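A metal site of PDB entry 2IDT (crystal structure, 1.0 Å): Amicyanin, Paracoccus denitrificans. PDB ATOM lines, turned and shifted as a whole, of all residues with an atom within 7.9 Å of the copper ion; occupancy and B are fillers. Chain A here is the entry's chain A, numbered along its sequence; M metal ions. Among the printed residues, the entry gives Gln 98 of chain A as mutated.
A ring nitrogen (NE2) of His 53 lies close to O of MHO 51, at 3.5 Å.
The side-chain carboxylate (OE1) of Glu 49 lies within hydrogen-bond range of a ring nitrogen (NE2) of His 53.
A ring nitrogen (NE2) of His 95 is in hydrogen-bond range of OD1 of MHO 51, at 2.7 Å.
NE2 of Gln 98 lies within hydrogen-bond range of O of Met 28, at 2.8 Å.
N of Asn 54 sits close to SG of Cys 92.
The side-chain hydroxyl of Tyr 30 is in hydrogen-bond range of the backbone NH of Cys 92 (3.2 Å).
Within 4 Å of the copper ion: His 53, Cys 92, His 95 and Gln 98.
The copper ion is bound by ND1 of His 53 (2.0 Å), ND1 of His 95 (2.0 Å), OE1 of Gln 98 (2.1 Å) and SG of Cys 92 (2.2 Å).
The copper ion has four donor atoms within binding distance.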
ATOM      1  N   ILE A  25     -10.822  21.347 -22.208  1.00  0.00           N
ATOM      2  CA  ILE A  25     -10.190  21.208 -20.928  1.00  0.00           C
ATOM      3  C   ILE A  25     -11.291  20.794 -19.929  1.00  0.00           C
ATOM      4  O   ILE A  25     -12.228  21.603 -19.669  1.00  0.00           O
ATOM      5  CB  ILE A  25      -9.490  22.526 -20.472  1.00  0.00           C
ATOM      6  CG1 ILE A  25      -8.617  23.098 -21.588  1.00  0.00           C
ATOM      7  CG2 ILE A  25      -8.674  22.275 -19.219  1.00  0.00           C
ATOM      8  CD1 ILE A  25      -8.027  24.471 -21.282  1.00  0.00           C
ATOM      9  N   MET A  28      -9.988  18.182 -15.343  1.00  0.00           N
ATOM     10  CA  MET A  28      -8.650  18.684 -14.935  1.00  0.00           C
ATOM     11  C   MET A  28      -7.554  18.189 -15.891  1.00  0.00           C
ATOM     12  O   MET A  28      -6.419  17.977 -15.494  1.00  0.00           O
ATOM     13  CB  MET A  28      -8.254  18.402 -13.475  1.00  0.00           C
ATOM     14  CG  MET A  28      -8.579  19.458 -12.453  1.00  0.00           C
ATOM     15  SD  MET A  28      -8.177  21.193 -12.263  1.00  0.00           S
ATOM     16  CE  MET A  28      -6.456  21.214 -11.822  1.00  0.00           C
ATOM     17  N   LYS A  29      -7.838  18.037 -17.178  1.00  0.00           N
ATOM     18  CA  LYS A  29      -6.848  17.637 -18.159  1.00  0.00           C
ATOM     19  C   LYS A  29      -7.146  18.291 -19.469  1.00  0.00           C
ATOM     20  O   LYS A  29      -8.304  18.701 -19.787  1.00  0.00           O
ATOM     21  CB  LYS A  29      -6.878  16.127 -18.344  1.00  0.00           C
ATOM     22  CG  LYS A  29      -6.538  15.316 -17.116  1.00  0.00           C
ATOM     23  CD  LYS A  29      -6.815  13.837 -17.371  1.00  0.00           C
ATOM     24  CE  LYS A  29      -6.774  13.079 -16.073  1.00  0.00           C
ATOM     25  NZ  LYS A  29      -7.862  12.109 -15.825  1.00  0.00           N
ATOM     26  N   TYR A  30      -6.115  18.378 -20.308  1.00  0.00           N
ATOM     27  CA  TYR A  30      -6.354  18.659 -21.746  1.00  0.00           C
ATOM     28  C   TYR A  30      -6.832  17.346 -22.353  1.00  0.00           C
ATOM     29  O   TYR A  30      -6.103  16.358 -22.363  1.00  0.00           O
ATOM     30  CB  TYR A  30      -5.053  19.093 -22.387  1.00  0.00           C
ATOM     31  CG  TYR A  30      -4.445  20.340 -21.834  1.00  0.00           C
ATOM     32  CD1 TYR A  30      -5.096  21.580 -21.953  1.00  0.00           C
ATOM     33  CD2 TYR A  30      -3.215  20.346 -21.158  1.00  0.00           C
ATOM     34  CE1 TYR A  30      -4.554  22.760 -21.436  1.00  0.00           C
ATOM     35  CE2 TYR A  30      -2.666  21.514 -20.671  1.00  0.00           C
ATOM     36  CZ  TYR A  30      -3.319  22.701 -20.794  1.00  0.00           C
ATOM     37  OH  TYR A  30      -2.691  23.830 -20.333  1.00  0.00           O
ATOM     38  N   ASN A  47     -12.183  25.920 -22.026  1.00  0.00           N
ATOM     39  CA  ASN A  47     -12.279  25.473 -20.620  1.00  0.00           C
ATOM     40  C   ASN A  47     -13.727  25.118 -20.311  1.00  0.00           C
ATOM     41  O   ASN A  47     -14.620  25.961 -20.423  1.00  0.00           O
ATOM     42  CB  ASN A  47     -11.803  26.584 -19.690  1.00  0.00           C
ATOM     43  CG  ASN A  47     -11.784  26.102 -18.254  1.00  0.00           C
ATOM     44  OD1 ASN A  47     -11.966  24.933 -17.980  1.00  0.00           O
ATOM     45  ND2 ASN A  47     -11.535  27.068 -17.346  1.00  0.00           N
ATOM     46  N   GLU A  49     -14.600  23.886 -17.237  1.00  0.00           N
ATOM     47  CA  GLU A  49     -14.649  23.764 -15.785  1.00  0.00           C
ATOM     48  C   GLU A  49     -14.655  25.106 -15.057  1.00  0.00           C
ATOM     49  O   GLU A  49     -14.187  26.092 -15.531  1.00  0.00           O
ATOM     50  CB  GLU A  49     -13.343  23.079 -15.275  1.00  0.00           C
ATOM     51  CG  GLU A  49     -13.022  21.762 -15.875  1.00  0.00           C
ATOM     52  CD  GLU A  49     -11.999  20.993 -15.099  1.00  0.00           C
ATOM     53  OE1 GLU A  49     -10.868  21.420 -14.857  1.00  0.00           O
ATOM     54  OE2 GLU A  49     -12.371  19.836 -14.739  1.00  0.00           O
ATOM     55  N   MHO A  51     -12.782  25.836 -12.441  1.00  0.00           N
ATOM     56  CA  MHO A  51     -11.408  26.262 -12.217  1.00  0.00           C
ATOM     57  CB  MHO A  51     -10.630  24.997 -11.823  1.00  0.00           C
ATOM     58  CG  MHO A  51      -9.131  25.257 -11.592  1.00  0.00           C
ATOM     59  SD  MHO A  51      -8.788  26.382 -10.263  1.00  0.00           S
ATOM     60  CE  MHO A  51      -9.280  25.358  -8.891  1.00  0.00           C
ATOM     61  C   MHO A  51     -10.812  26.896 -13.446  1.00  0.00           C
ATOM     62  O   MHO A  51     -10.888  26.244 -14.518  1.00  0.00           O
ATOM     63  OD1 MHO A  51      -7.170  26.381 -10.109  1.00  0.00           O
ATOM     64  N   PRO A  52     -10.223  28.069 -13.446  1.00  0.00           N
ATOM     65  CA  PRO A  52      -9.574  28.624 -14.632  1.00  0.00           C
ATOM     66  C   PRO A  52      -8.362  27.773 -15.059  1.00  0.00           C
ATOM     67  O   PRO A  52      -7.658  27.190 -14.255  1.00  0.00           O
ATOM     68  CB  PRO A  52      -9.125  30.017 -14.189  1.00  0.00           C
ATOM     69  CG  PRO A  52     -10.094  30.381 -13.074  1.00  0.00           C
ATOM     70  CD  PRO A  52     -10.184  29.048 -12.302  1.00  0.00           C
ATOM     71  N   HIS A  53      -8.103  27.832 -16.371  1.00  0.00           N
ATOM     72  CA  HIS A  53      -6.964  27.170 -16.982  1.00  0.00           C
ATOM     73  C   HIS A  53      -6.417  28.046 -18.106  1.00  0.00           C
ATOM     74  O   HIS A  53      -7.106  28.898 -18.639  1.00  0.00           O
ATOM     75  CB  HIS A  53      -7.387  25.824 -17.610  1.00  0.00           C
ATOM     76  CG  HIS A  53      -7.903  24.824 -16.636  1.00  0.00           C
ATOM     77  ND1 HIS A  53      -7.093  24.063 -15.779  1.00  0.00           N
ATOM     78  CD2 HIS A  53      -9.177  24.381 -16.444  1.00  0.00           C
ATOM     79  CE1 HIS A  53      -7.869  23.245 -15.075  1.00  0.00           C
ATOM     80  NE2 HIS A  53      -9.102  23.427 -15.483  1.00  0.00           N
ATOM     81  N   ASN A  54      -5.169  27.774 -18.483  1.00  0.00           N
ATOM     82  CA  ASN A  54      -4.612  28.427 -19.655  1.00  0.00           C
ATOM     83  C   ASN A  54      -3.794  27.375 -20.443  1.00  0.00           C
ATOM     84  O   ASN A  54      -3.833  26.202 -20.142  1.00  0.00           O
ATOM     85  CB  ASN A  54      -3.779  29.697 -19.357  1.00  0.00           C
ATOM     86  CG  ASN A  54      -2.442  29.356 -18.726  1.00  0.00           C
ATOM     87  OD1 ASN A  54      -2.241  28.252 -18.256  1.00  0.00           O
ATOM     88  ND2 ASN A  54      -1.557  30.357 -18.727  1.00  0.00           N
ATOM     89  N   VAL A  55      -3.057  27.880 -21.430  1.00  0.00           N
ATOM     90  CA  VAL A  55      -1.982  27.109 -22.042  1.00  0.00           C
ATOM     91  C   VAL A  55      -0.719  27.981 -21.980  1.00  0.00           C
ATOM     92  O   VAL A  55      -0.777  29.189 -22.142  1.00  0.00           O
ATOM     93  CB  VAL A  55      -2.284  26.722 -23.523  1.00  0.00           C
ATOM     94  CG1 VAL A  55      -3.437  25.737 -23.519  1.00  0.00           C
ATOM     95  CG2 VAL A  55      -2.540  27.911 -24.405  1.00  0.00           C
ATOM     96  N   MET A  71      -5.849  33.452 -18.723  1.00  0.00           N
ATOM     97  CA  MET A  71      -6.649  32.464 -17.997  1.00  0.00           C
ATOM     98  C   MET A  71      -8.056  32.470 -18.535  1.00  0.00           C
ATOM     99  O   MET A  71      -8.723  33.499 -18.661  1.00  0.00           O
ATOM    100  CB  MET A  71      -6.692  32.879 -16.499  1.00  0.00           C
ATOM    101  CG  MET A  71      -5.317  32.854 -15.853  1.00  0.00           C
ATOM    102  SD  MET A  71      -4.346  31.330 -16.078  1.00  0.00           S
ATOM    103  CE  MET A  71      -5.404  30.123 -15.363  1.00  0.00           C
ATOM    104  N   HIS A  91       1.875  23.505 -20.982  1.00  0.00           N
ATOM    105  CA  HIS A  91       1.305  23.132 -19.707  1.00  0.00           C
ATOM    106  C   HIS A  91       0.336  24.216 -19.275  1.00  0.00           C
ATOM    107  O   HIS A  91       0.288  25.302 -19.843  1.00  0.00           O
ATOM    108  CB  HIS A  91       2.400  22.885 -18.640  1.00  0.00           C
ATOM    109  CG  HIS A  91       3.148  24.112 -18.224  1.00  0.00           C
ATOM    110  ND1 HIS A  91       4.143  24.668 -18.948  1.00  0.00           N
ATOM    111  CD2 HIS A  91       2.934  24.910 -17.134  1.00  0.00           C
ATOM    112  CE1 HIS A  91       4.590  25.772 -18.306  1.00  0.00           C
ATOM    113  NE2 HIS A  91       3.854  25.931 -17.213  1.00  0.00           N
ATOM    114  N   CYS A  92      -0.359  23.936 -18.181  1.00  0.00           N
ATOM    115  CA  CYS A  92      -1.238  24.954 -17.596  1.00  0.00           C
ATOM    116  C   CYS A  92      -0.484  25.690 -16.467  1.00  0.00           C
ATOM    117  O   CYS A  92       0.045  25.033 -15.577  1.00  0.00           O
ATOM    118  CB  CYS A  92      -2.464  24.223 -17.009  1.00  0.00           C
ATOM    119  SG  CYS A  92      -3.629  25.419 -16.335  1.00  0.00           S
ATOM    120  N   THR A  93      -0.438  27.023 -16.533  1.00  0.00           N
ATOM    121  CA  THR A  93       0.388  27.772 -15.573  1.00  0.00           C
ATOM    122  C   THR A  93       0.025  27.443 -14.131  1.00  0.00           C
ATOM    123  O   THR A  93       0.917  27.119 -13.324  1.00  0.00           O
ATOM    124  CB  THR A  93       0.290  29.273 -15.858  1.00  0.00           C
ATOM    125  OG1 THR A  93       0.726  29.549 -17.184  1.00  0.00           O
ATOM    126  CG2 THR A  93       1.100  30.052 -14.815  1.00  0.00           C
ATOM    127  N   PRO A  94      -1.245  27.577 -13.704  1.00  0.00           N
ATOM    128  CA  PRO A  94      -1.517  27.272 -12.295  1.00  0.00           C
ATOM    129  C   PRO A  94      -1.469  25.789 -11.963  1.00  0.00           C
ATOM    130  O   PRO A  94      -1.403  25.410 -10.763  1.00  0.00           O
ATOM    131  CB  PRO A  94      -2.971  27.789 -12.103  1.00  0.00           C
ATOM    132  CG  PRO A  94      -3.540  27.710 -13.474  1.00  0.00           C
ATOM    133  CD  PRO A  94      -2.420  28.120 -14.384  1.00  0.00           C
ATOM    134  N   HIS A  95      -1.519  24.916 -13.001  1.00  0.00           N
ATOM    135  CA  HIS A  95      -1.554  23.453 -12.792  1.00  0.00           C
ATOM    136  C   HIS A  95      -0.514  22.760 -13.626  1.00  0.00           C
ATOM    137  O   HIS A  95      -0.790  22.152 -14.680  1.00  0.00           O
ATOM    138  CB  HIS A  95      -2.923  22.907 -13.191  1.00  0.00           C
ATOM    139  CG  HIS A  95      -4.065  23.627 -12.569  1.00  0.00           C
ATOM    140  ND1 HIS A  95      -5.029  24.184 -13.399  1.00  0.00           N
ATOM    141  CD2 HIS A  95      -4.389  23.912 -11.287  1.00  0.00           C
ATOM    142  CE1 HIS A  95      -5.906  24.764 -12.608  1.00  0.00           C
ATOM    143  NE2 HIS A  95      -5.552  24.621 -11.323  1.00  0.00           N
ATOM    144  N   PRO A  96       0.763  22.893 -13.267  1.00  0.00           N
ATOM    145  CA  PRO A  96       1.804  22.379 -14.176  1.00  0.00           C
ATOM    146  C   PRO A  96       1.822  20.869 -14.376  1.00  0.00           C
ATOM    147  O   PRO A  96       2.439  20.393 -15.327  1.00  0.00           O
ATOM    148  CB  PRO A  96       3.097  22.885 -13.556  1.00  0.00           C
ATOM    149  CG  PRO A  96       2.749  23.125 -12.104  1.00  0.00           C
ATOM    150  CD  PRO A  96       1.318  23.636 -12.142  1.00  0.00           C
ATOM    151  N   PHE A  97       1.108  20.119 -13.541  1.00  0.00           N
ATOM    152  CA  PHE A  97       0.926  18.710 -13.806  1.00  0.00           C
ATOM    153  C   PHE A  97       0.069  18.445 -15.019  1.00  0.00           C
ATOM    154  O   PHE A  97      -0.009  17.320 -15.506  1.00  0.00           O
ATOM    155  CB  PHE A  97       0.331  18.024 -12.551  1.00  0.00           C
ATOM    156  CG  PHE A  97      -0.879  18.798 -11.986  1.00  0.00           C
ATOM    157  CD1 PHE A  97      -2.121  18.545 -12.479  1.00  0.00           C
ATOM    158  CD2 PHE A  97      -0.700  19.735 -10.954  1.00  0.00           C
ATOM    159  CE1 PHE A  97      -3.296  19.144 -12.008  1.00  0.00           C
ATOM    160  CE2 PHE A  97      -1.841  20.403 -10.487  1.00  0.00           C
ATOM    161  CZ  PHE A  97      -3.092  20.110 -11.011  1.00  0.00           C
ATOM    162  N   GLN A  98      -0.608  19.434 -15.568  1.00  0.00           N
ATOM    163  CA  GLN A  98      -1.471  19.334 -16.743  1.00  0.00           C
ATOM    164  C   GLN A  98      -0.683  19.729 -17.984  1.00  0.00           C
ATOM    165  O   GLN A  98      -0.290  20.868 -18.134  1.00  0.00           O
ATOM    166  CB  GLN A  98      -2.671  20.289 -16.723  1.00  0.00           C
ATOM    167  CG  GLN A  98      -3.778  19.901 -15.785  1.00  0.00           C
ATOM    168  CD  GLN A  98      -4.765  20.993 -15.455  1.00  0.00           C
ATOM    169  OE1 GLN A  98      -4.690  22.167 -15.823  1.00  0.00           O
ATOM    170  NE2 GLN A  98      -5.747  20.600 -14.661  1.00  0.00           N
HETATM  171 CU    CU M   1      -5.151  24.196 -15.418  1.00  0.00          CU
